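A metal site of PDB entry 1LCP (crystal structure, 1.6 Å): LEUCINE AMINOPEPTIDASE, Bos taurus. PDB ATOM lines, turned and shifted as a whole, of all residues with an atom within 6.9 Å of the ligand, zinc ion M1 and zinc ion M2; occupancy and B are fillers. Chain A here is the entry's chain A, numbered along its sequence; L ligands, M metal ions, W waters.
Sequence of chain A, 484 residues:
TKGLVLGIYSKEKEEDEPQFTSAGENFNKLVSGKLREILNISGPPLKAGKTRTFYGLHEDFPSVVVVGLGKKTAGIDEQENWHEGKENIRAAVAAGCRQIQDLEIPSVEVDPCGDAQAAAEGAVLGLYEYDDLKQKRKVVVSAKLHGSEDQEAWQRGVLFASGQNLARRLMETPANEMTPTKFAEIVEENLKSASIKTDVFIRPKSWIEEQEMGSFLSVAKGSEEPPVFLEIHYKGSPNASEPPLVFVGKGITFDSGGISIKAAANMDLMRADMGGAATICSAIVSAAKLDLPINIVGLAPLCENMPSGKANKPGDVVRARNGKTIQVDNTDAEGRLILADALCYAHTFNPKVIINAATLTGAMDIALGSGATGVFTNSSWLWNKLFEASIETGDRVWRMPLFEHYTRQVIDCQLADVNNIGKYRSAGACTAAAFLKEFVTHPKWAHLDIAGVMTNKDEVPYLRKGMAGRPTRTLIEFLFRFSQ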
ATOM      1  N   LYS A 250      -9.522   5.814 -15.643  1.00  0.00           N
ATOM      2  CA  LYS A 250      -9.502   5.871 -17.125  1.00  0.00           C
ATOM      3  C   LYS A 250     -10.781   5.194 -17.680  1.00  0.00           C
ATOM      4  O   LYS A 250     -11.022   4.007 -17.429  1.00  0.00           O
ATOM      5  CB  LYS A 250      -8.257   5.138 -17.661  1.00  0.00           C
ATOM      6  CG  LYS A 250      -8.200   4.991 -19.185  1.00  0.00           C
ATOM      7  CD  LYS A 250      -7.029   4.100 -19.640  1.00  0.00           C
ATOM      8  CE  LYS A 250      -7.093   3.767 -21.147  1.00  0.00           C
ATOM      9  NZ  LYS A 250      -5.959   2.880 -21.600  1.00  0.00           N
ATOM     10  N   ILE A 252     -11.968   4.607 -21.098  1.00  0.00           N
ATOM     11  CA  ILE A 252     -12.037   4.409 -22.564  1.00  0.00           C
ATOM     12  C   ILE A 252     -12.989   3.212 -22.782  1.00  0.00           C
ATOM     13  O   ILE A 252     -12.613   2.068 -22.526  1.00  0.00           O
ATOM     14  CB  ILE A 252     -10.651   4.127 -23.180  1.00  0.00           C
ATOM     15  CG1 ILE A 252      -9.706   5.329 -23.023  1.00  0.00           C
ATOM     16  CG2 ILE A 252     -10.795   3.750 -24.653  1.00  0.00           C
ATOM     17  CD1 ILE A 252     -10.129   6.571 -23.808  1.00  0.00           C
ATOM     18  N   ASP A 255     -11.172   0.863 -27.085  1.00  0.00           N
ATOM     19  CA  ASP A 255      -9.901   1.358 -27.617  1.00  0.00           C
ATOM     20  C   ASP A 255      -9.489   0.611 -28.886  1.00  0.00           C
ATOM     21  O   ASP A 255      -9.009  -0.531 -28.811  1.00  0.00           O
ATOM     22  CB  ASP A 255      -8.806   1.206 -26.555  1.00  0.00           C
ATOM     23  CG  ASP A 255      -7.485   1.891 -26.948  1.00  0.00           C
ATOM     24  OD1 ASP A 255      -7.448   2.657 -27.951  1.00  0.00           O
ATOM     25  OD2 ASP A 255      -6.481   1.658 -26.242  1.00  0.00           O
ATOM     26  N   SER A 256      -9.664   1.260 -30.036  1.00  0.00           N
ATOM     27  CA  SER A 256      -9.280   0.678 -31.328  1.00  0.00           C
ATOM     28  C   SER A 256      -7.844   1.116 -31.662  1.00  0.00           C
ATOM     29  O   SER A 256      -7.267   0.624 -32.638  1.00  0.00           O
ATOM     30  CB  SER A 256     -10.196   1.189 -32.439  1.00  0.00           C
ATOM     31  OG  SER A 256      -9.842   2.514 -32.832  1.00  0.00           O
ATOM     32  N   GLY A 257      -7.320   2.078 -30.907  1.00  0.00           N
ATOM     33  CA  GLY A 257      -5.999   2.617 -31.166  1.00  0.00           C
ATOM     34  C   GLY A 257      -6.058   3.913 -31.978  1.00  0.00           C
ATOM     35  O   GLY A 257      -5.139   4.740 -31.914  1.00  0.00           O
ATOM     36  N   GLY A 258      -7.153   4.099 -32.710  1.00  0.00           N
ATOM     37  CA  GLY A 258      -7.313   5.291 -33.539  1.00  0.00           C
ATOM     38  C   GLY A 258      -6.503   5.161 -34.822  1.00  0.00           C
ATOM     39  O   GLY A 258      -6.410   4.068 -35.383  1.00  0.00           O
ATOM     40  N   SER A 260      -3.346   5.224 -35.114  1.00  0.00           N
ATOM     41  CA  SER A 260      -2.272   4.282 -34.782  1.00  0.00           C
ATOM     42  C   SER A 260      -3.048   2.988 -34.391  1.00  0.00           C
ATOM     43  O   SER A 260      -2.992   2.523 -33.239  1.00  0.00           O
ATOM     44  CB  SER A 260      -1.459   4.808 -33.588  1.00  0.00           C
ATOM     45  OG  SER A 260      -0.890   6.100 -33.831  1.00  0.00           O
ATOM     46  N   LYS A 262      -4.811  -0.651 -33.715  1.00  0.00           N
ATOM     47  CA  LYS A 262      -4.381  -1.911 -33.101  1.00  0.00           C
ATOM     48  C   LYS A 262      -4.515  -3.061 -34.081  1.00  0.00           C
ATOM     49  O   LYS A 262      -5.224  -2.949 -35.087  1.00  0.00           O
ATOM     50  CB  LYS A 262      -5.262  -2.234 -31.895  1.00  0.00           C
ATOM     51  CG  LYS A 262      -5.032  -1.357 -30.677  1.00  0.00           C
ATOM     52  CD  LYS A 262      -5.875  -1.853 -29.499  1.00  0.00           C
ATOM     53  CE  LYS A 262      -5.700  -0.978 -28.267  1.00  0.00           C
ATOM     54  NZ  LYS A 262      -4.284  -0.900 -27.813  1.00  0.00           N
ATOM     55  N   MET A 270     -10.626  -4.922 -25.566  1.00  0.00           N
ATOM     56  CA  MET A 270     -10.524  -3.485 -25.357  1.00  0.00           C
ATOM     57  C   MET A 270     -11.852  -2.840 -24.933  1.00  0.00           C
ATOM     58  O   MET A 270     -11.894  -1.629 -24.668  1.00  0.00           O
ATOM     59  CB  MET A 270      -9.884  -2.798 -26.589  1.00  0.00           C
ATOM     60  CG  MET A 270      -8.399  -3.203 -26.828  1.00  0.00           C
ATOM     61  SD  MET A 270      -7.304  -2.841 -25.388  1.00  0.00           S
ATOM     62  CE  MET A 270      -7.155  -4.436 -24.660  1.00  0.00           C
ATOM     63  N   ASP A 273     -11.354  -1.369 -21.565  1.00  0.00           N
ATOM     64  CA  ASP A 273     -10.377  -0.283 -21.382  1.00  0.00           C
ATOM     65  C   ASP A 273     -10.910   0.840 -20.476  1.00  0.00           C
ATOM     66  O   ASP A 273     -10.290   1.893 -20.321  1.00  0.00           O
ATOM     67  CB  ASP A 273      -9.902   0.267 -22.732  1.00  0.00           C
ATOM     68  CG  ASP A 273      -8.482   0.832 -22.668  1.00  0.00           C
ATOM     69  OD1 ASP A 273      -7.671   0.384 -21.812  1.00  0.00           O
ATOM     70  OD2 ASP A 273      -8.187   1.727 -23.478  1.00  0.00           O
ATOM     71  N   ASN A 305     -11.999   5.560 -28.486  1.00  0.00           N
ATOM     72  CA  ASN A 305     -10.798   5.945 -29.250  1.00  0.00           C
ATOM     73  C   ASN A 305     -10.972   5.232 -30.599  1.00  0.00           C
ATOM     74  O   ASN A 305     -10.699   4.038 -30.722  1.00  0.00           O
ATOM     75  CB  ASN A 305      -9.514   5.486 -28.522  1.00  0.00           C
ATOM     76  CG  ASN A 305      -8.236   6.012 -29.191  1.00  0.00           C
ATOM     77  OD1 ASN A 305      -7.175   5.380 -29.088  1.00  0.00           O
ATOM     78  ND2 ASN A 305      -8.319   7.152 -29.835  1.00  0.00           N
ATOM     79  N   ASN A 330       1.765   8.801 -30.813  1.00  0.00           N
ATOM     80  CA  ASN A 330       1.046   7.536 -31.039  1.00  0.00           C
ATOM     81  C   ASN A 330      -0.366   7.724 -30.458  1.00  0.00           C
ATOM     82  O   ASN A 330      -0.536   7.859 -29.247  1.00  0.00           O
ATOM     83  CB  ASN A 330       1.775   6.383 -30.343  1.00  0.00           C
ATOM     84  CG  ASN A 330       1.226   5.016 -30.720  1.00  0.00           C
ATOM     85  OD1 ASN A 330       1.949   4.138 -31.232  1.00  0.00           O
ATOM     86  ND2 ASN A 330      -0.046   4.811 -30.455  1.00  0.00           N
ATOM     87  N   THR A 331      -1.375   7.695 -31.336  1.00  0.00           N
ATOM     88  CA  THR A 331      -2.767   7.913 -30.913  1.00  0.00           C
ATOM     89  C   THR A 331      -3.332   6.819 -30.001  1.00  0.00           C
ATOM     90  O   THR A 331      -4.367   7.003 -29.358  1.00  0.00           O
ATOM     91  CB  THR A 331      -3.716   8.117 -32.137  1.00  0.00           C
ATOM     92  OG1 THR A 331      -3.845   6.894 -32.884  1.00  0.00           O
ATOM     93  CG2 THR A 331      -3.148   9.213 -33.090  1.00  0.00           C
ATOM     94  N   ASP A 332      -2.647   5.667 -29.961  1.00  0.00           N
ATOM     95  CA  ASP A 332      -3.046   4.532 -29.127  1.00  0.00           C
ATOM     96  C   ASP A 332      -2.539   4.655 -27.674  1.00  0.00           C
ATOM     97  O   ASP A 332      -2.776   3.785 -26.833  1.00  0.00           O
ATOM     98  CB  ASP A 332      -2.592   3.224 -29.786  1.00  0.00           C
ATOM     99  CG  ASP A 332      -3.277   1.986 -29.207  1.00  0.00           C
ATOM    100  OD1 ASP A 332      -4.326   2.094 -28.541  1.00  0.00           O
ATOM    101  OD2 ASP A 332      -2.749   0.880 -29.456  1.00  0.00           O
ATOM    102  N   ALA A 333      -1.762   5.684 -27.386  1.00  0.00           N
ATOM    103  CA  ALA A 333      -1.299   5.920 -26.018  1.00  0.00           C
ATOM    104  C   ALA A 333      -2.294   6.986 -25.543  1.00  0.00           C
ATOM    105  O   ALA A 333      -1.914   8.084 -25.102  1.00  0.00           O
ATOM    106  CB  ALA A 333       0.133   6.452 -26.001  1.00  0.00           C
ATOM    107  N   GLU A 334      -3.581   6.651 -25.622  1.00  0.00           N
ATOM    108  CA  GLU A 334      -4.637   7.592 -25.286  1.00  0.00           C
ATOM    109  C   GLU A 334      -5.018   7.711 -23.822  1.00  0.00           C
ATOM    110  O   GLU A 334      -5.590   8.743 -23.417  1.00  0.00           O
ATOM    111  CB  GLU A 334      -5.882   7.290 -26.135  1.00  0.00           C
ATOM    112  CG  GLU A 334      -6.851   6.225 -25.590  1.00  0.00           C
ATOM    113  CD  GLU A 334      -6.244   4.836 -25.467  1.00  0.00           C
ATOM    114  OE1 GLU A 334      -5.450   4.448 -26.344  1.00  0.00           O
ATOM    115  OE2 GLU A 334      -6.594   4.133 -24.500  1.00  0.00           O
ATOM    116  N   GLY A 335      -4.772   6.662 -23.043  1.00  0.00           N
ATOM    117  CA  GLY A 335      -5.130   6.683 -21.627  1.00  0.00           C
ATOM    118  C   GLY A 335      -4.439   7.807 -20.880  1.00  0.00           C
ATOM    119  O   GLY A 335      -5.080   8.536 -20.108  1.00  0.00           O
ATOM    120  N   ARG A 336      -3.158   7.993 -21.132  1.00  0.00           N
ATOM    121  CA  ARG A 336      -2.427   9.054 -20.450  1.00  0.00           C
ATOM    122  C   ARG A 336      -2.912  10.444 -20.877  1.00  0.00           C
ATOM    123  O   ARG A 336      -2.861  11.396 -20.082  1.00  0.00           O
ATOM    124  CB  ARG A 336      -0.911   8.887 -20.647  1.00  0.00           C
ATOM    125  CG  ARG A 336      -0.388   9.121 -22.023  1.00  0.00           C
ATOM    126  CD  ARG A 336       1.032   8.572 -22.134  1.00  0.00           C
ATOM    127  NE  ARG A 336       1.030   7.117 -22.277  1.00  0.00           N
ATOM    128  CZ  ARG A 336       2.121   6.357 -22.330  1.00  0.00           C
ATOM    129  NH1 ARG A 336       3.342   6.879 -22.213  1.00  0.00           N
ATOM    130  NH2 ARG A 336       1.994   5.048 -22.485  1.00  0.00           N
ATOM    131  N   THR A 359      -6.167   0.837 -17.030  1.00  0.00           N
ATOM    132  CA  THR A 359      -5.689  -0.326 -17.783  1.00  0.00           C
ATOM    133  C   THR A 359      -4.735   0.421 -18.735  1.00  0.00           C
ATOM    134  O   THR A 359      -4.979   0.542 -19.931  1.00  0.00           O
ATOM    135  CB  THR A 359      -6.876  -0.971 -18.564  1.00  0.00           C
ATOM    136  OG1 THR A 359      -7.688   0.062 -19.154  1.00  0.00           O
ATOM    137  CG2 THR A 359      -7.767  -1.797 -17.606  1.00  0.00           C
ATOM    138  N   LEU A 360      -3.645   0.954 -18.173  1.00  0.00           N
ATOM    139  CA  LEU A 360      -2.738   1.812 -18.924  1.00  0.00           C
ATOM    140  C   LEU A 360      -1.750   1.287 -19.958  1.00  0.00           C
ATOM    141  O   LEU A 360      -1.624   1.877 -21.042  1.00  0.00           O
ATOM    142  CB  LEU A 360      -2.009   2.763 -17.961  1.00  0.00           C
ATOM    143  CG  LEU A 360      -1.526   4.088 -18.577  1.00  0.00           C
ATOM    144  CD1 LEU A 360      -2.741   4.937 -18.974  1.00  0.00           C
ATOM    145  CD2 LEU A 360      -0.650   4.873 -17.600  1.00  0.00           C
ATOM    146  N   THR A 361      -1.019   0.222 -19.651  1.00  0.00           N
ATOM    147  CA  THR A 361      -0.021  -0.254 -20.602  1.00  0.00           C
ATOM    148  C   THR A 361       0.105  -1.763 -20.788  1.00  0.00           C
ATOM    149  O   THR A 361      -0.023  -2.530 -19.839  1.00  0.00           O
ATOM    150  CB  THR A 361       1.399   0.271 -20.177  1.00  0.00           C
ATOM    151  OG1 THR A 361       1.779  -0.333 -18.928  1.00  0.00           O
ATOM    152  CG2 THR A 361       1.436   1.811 -20.059  1.00  0.00           C
ATOM    153  N   GLY A 362       0.391  -2.178 -22.016  1.00  0.00           N
ATOM    154  CA  GLY A 362       0.612  -3.593 -22.254  1.00  0.00           C
ATOM    155  C   GLY A 362       1.905  -3.964 -21.519  1.00  0.00           C
ATOM    156  O   GLY A 362       2.077  -5.104 -21.075  1.00  0.00           O
ATOM    157  N   ALA A 363       2.801  -2.990 -21.374  1.00  0.00           N
ATOM    158  CA  ALA A 363       4.079  -3.197 -20.684  1.00  0.00           C
ATOM    159  C   ALA A 363       3.885  -3.705 -19.251  1.00  0.00           C
ATOM    160  O   ALA A 363       4.659  -4.543 -18.780  1.00  0.00           O
ATOM    161  CB  ALA A 363       4.898  -1.906 -20.682  1.00  0.00           C
ATOM    162  N   ASP A 365       1.501  -5.576 -18.258  1.00  0.00           N
ATOM    163  CA  ASP A 365       1.158  -6.996 -18.369  1.00  0.00           C
ATOM    164  C   ASP A 365       2.424  -7.839 -18.595  1.00  0.00           C
ATOM    165  O   ASP A 365       2.589  -8.917 -18.018  1.00  0.00           O
ATOM    166  CB  ASP A 365       0.160  -7.226 -19.502  1.00  0.00           C
ATOM    167  CG  ASP A 365      -0.250  -8.692 -19.601  1.00  0.00           C
ATOM    168  OD1 ASP A 365      -0.810  -9.224 -18.622  1.00  0.00           O
ATOM    169  OD2 ASP A 365       0.040  -9.320 -20.624  1.00  0.00           O
ATOM    170  N   ASP A 449      -1.656   0.781 -12.247  1.00  0.00           N
ATOM    171  CA  ASP A 449      -1.756   0.306 -13.628  1.00  0.00           C
ATOM    172  C   ASP A 449      -2.318  -1.123 -13.487  1.00  0.00           C
ATOM    173  O   ASP A 449      -1.613  -2.042 -13.048  1.00  0.00           O
ATOM    174  CB  ASP A 449      -0.374   0.292 -14.325  1.00  0.00           C
ATOM    175  CG  ASP A 449      -0.472   0.041 -15.842  1.00  0.00           C
ATOM    176  OD1 ASP A 449      -1.481  -0.532 -16.323  1.00  0.00           O
ATOM    177  OD2 ASP A 449       0.475   0.440 -16.567  1.00  0.00           O
ATOM    178  N   ILE A 450      -3.592  -1.275 -13.839  1.00  0.00           N
ATOM    179  CA  ILE A 450      -4.302  -2.555 -13.729  1.00  0.00           C
ATOM    180  C   ILE A 450      -4.431  -3.351 -15.038  1.00  0.00           C
ATOM    181  O   ILE A 450      -5.184  -4.324 -15.103  1.00  0.00           O
ATOM    182  CB  ILE A 450      -5.720  -2.341 -13.120  1.00  0.00           C
ATOM    183  CG1 ILE A 450      -6.593  -1.494 -14.062  1.00  0.00           C
ATOM    184  CG2 ILE A 450      -5.618  -1.679 -11.738  1.00  0.00           C
ATOM    185  CD1 ILE A 450      -8.076  -1.526 -13.726  1.00  0.00           C
ATOM    186  N   ALA A 451      -3.674  -2.961 -16.061  1.00  0.00           N
ATOM    187  CA  ALA A 451      -3.730  -3.656 -17.351  1.00  0.00           C
ATOM    188  C   ALA A 451      -3.514  -5.164 -17.239  1.00  0.00           C
ATOM    189  O   ALA A 451      -4.211  -5.951 -17.886  1.00  0.00           O
ATOM    190  CB  ALA A 451      -2.711  -3.048 -18.306  1.00  0.00           C
ATOM    191  N   GLY A 452      -2.565  -5.575 -16.400  1.00  0.00           N
ATOM    192  CA  GLY A 452      -2.277  -6.995 -16.217  1.00  0.00           C
ATOM    193  C   GLY A 452      -3.332  -7.811 -15.490  1.00  0.00           C
ATOM    194  O   GLY A 452      -3.402  -9.039 -15.663  1.00  0.00           O
ATOM    195  N   MET A 454      -6.654  -7.150 -15.792  1.00  0.00           N
ATOM    196  CA  MET A 454      -7.914  -6.874 -16.464  1.00  0.00           C
ATOM    197  C   MET A 454      -8.779  -8.149 -16.576  1.00  0.00           C
ATOM    198  O   MET A 454     -10.001  -8.115 -16.372  1.00  0.00           O
ATOM    199  CB  MET A 454      -7.664  -6.330 -17.876  1.00  0.00           C
ATOM    200  CG  MET A 454      -8.945  -6.182 -18.720  1.00  0.00           C
ATOM    201  SD  MET A 454      -8.729  -5.477 -20.387  1.00  0.00           S
ATOM    202  CE  MET A 454      -8.311  -6.917 -21.297  1.00  0.00           C
HETATM  203  C1  LIG L   1      -4.028   0.056 -23.474  1.00  0.00           C
HETATM  204  C2  LIG L   1      -3.524  -1.332 -23.871  1.00  0.00           C
HETATM  205  C3  LIG L   1      -4.168  -2.561 -23.155  1.00  0.00           C
HETATM  206  C4  LIG L   1      -4.101  -2.485 -21.640  1.00  0.00           C
HETATM  207  C5  LIG L   1      -3.561  -3.894 -23.629  1.00  0.00           C
HETATM  208  N1  LIG L   1      -5.481   0.118 -23.682  1.00  0.00           N
HETATM  209  P1  LIG L   1      -3.274   1.314 -24.538  1.00  0.00           P
HETATM  210  O1  LIG L   1      -3.995   2.645 -24.217  1.00  0.00           O
HETATM  211  O2  LIG L   1      -3.493   0.954 -26.049  1.00  0.00           O
HETATM  212  O3  LIG L   1      -1.770   1.363 -24.230  1.00  0.00           O
HETATM  213 ZN    ZN M   1      -6.154   2.301 -23.637  1.00  0.00          ZN
HETATM  214 ZN    ZN M   2      -4.637   2.630 -26.619  1.00  0.00          ZN
HETATM  215  O   HOH W   1       0.040  -0.496 -24.294  1.00  0.00           O
HETATM  216  O   HOH W   2      -0.186   3.485 -23.422  1.00  0.00           O
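Water W1 lies within hydrogen-bond range of O3 of the ligand (2.6 Å) and N of Gly 362 (2.9 Å). Water W2 lies within hydrogen-bond range of an oxygen (O3) of the ligand (2.8 Å), the guanidinium group of Arg 336 (2.8 Å) and the backbone carbonyl oxygen of Leu 360 (3.2 Å).
Four residues have an atom within 4 Å of zinc ion M1: Lys 250, Asp 255, Asp 273 and Glu 334.
The side-chain carboxylate (OE1) of Glu 334 sits close to the side-chain amide oxygen (OD1) of Asn 305 (3.4 Å). NZ of Lys 262 lies within salt-bridge range of OD2 of Asp 332. N of Ile 252 lies within hydrogen-bond range of O of Asp 273 (3.3 Å). The side-chain carboxylate (OD1) of Asp 255 lies close to the side-chain amide oxygen (OD1) of Asn 305. The side-chain carboxylate of Asp 255 is in hydrogen-bond range of the backbone NH of Gly 257 (3.0 Å). The backbone NH (N) of Lys 262 sits at hydrogen-bond distance from the backbone carbonyl oxygen (O) of Ser 256 (3.0 Å). The backbone NH of Leu 360 is in hydrogen-bond range of the side-chain carboxylate of Asp 449 (3.2 Å). The backbone NH of Ala 451 is in hydrogen-bond range of the side-chain carboxylate of Asp 449, at 3.3 Å.
O3 of the ligand lies close to O of Leu 360 (3.2 Å). CE of Met 270 touches C5 of the ligand (3.8 Å). O of Thr 359 touches C4 of the ligand (3.6 Å). CB of Ala 451 touches C4 of the ligand, at 3.7 Å. Hydrophobic or aromatic side chains within 4 Å of the ligand: Met 270 and Ala 451. Ten residues have an atom within 4 Å of the ligand: Lys 250, Asp 255, Lys 262, Met 270, Asp 273, Asp 332, Glu 334, Thr 359, Leu 360 and Ala 451.
Zinc ion M2 is bound by OE1 of Glu 334, OD1 of Asp 332, O2 of the ligand, OD2 of Asp 255, O of Asp 332 and O1 of the ligand.
OE2 of Glu 334 is bound to zinc ion M1, at 2.1 Å. The side-chain carboxylate (OD2) of Asp 273 is bound to zinc ion M1. Zinc ion M1 is bound by NZ of Lys 250 (2.1 Å). O1 of the ligand binds zinc ion M1, at 2.3 Å. Zinc ion M1 is bound by N1 of the ligand, 2.3 Å away. Zinc ion M1 has five donor atoms within binding distance. Slightly farther from zinc ion M1 lies the side-chain carboxylate (OD2) of Asp 255 (2.7 Å).
NZ of Lys 262 lies close to O2 of the ligand, 2.7 Å away.
Merely in contact with zinc ion M2: Lys 262. Of the 29 residues printed, 4 come within 4 Å of zinc ion M2.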
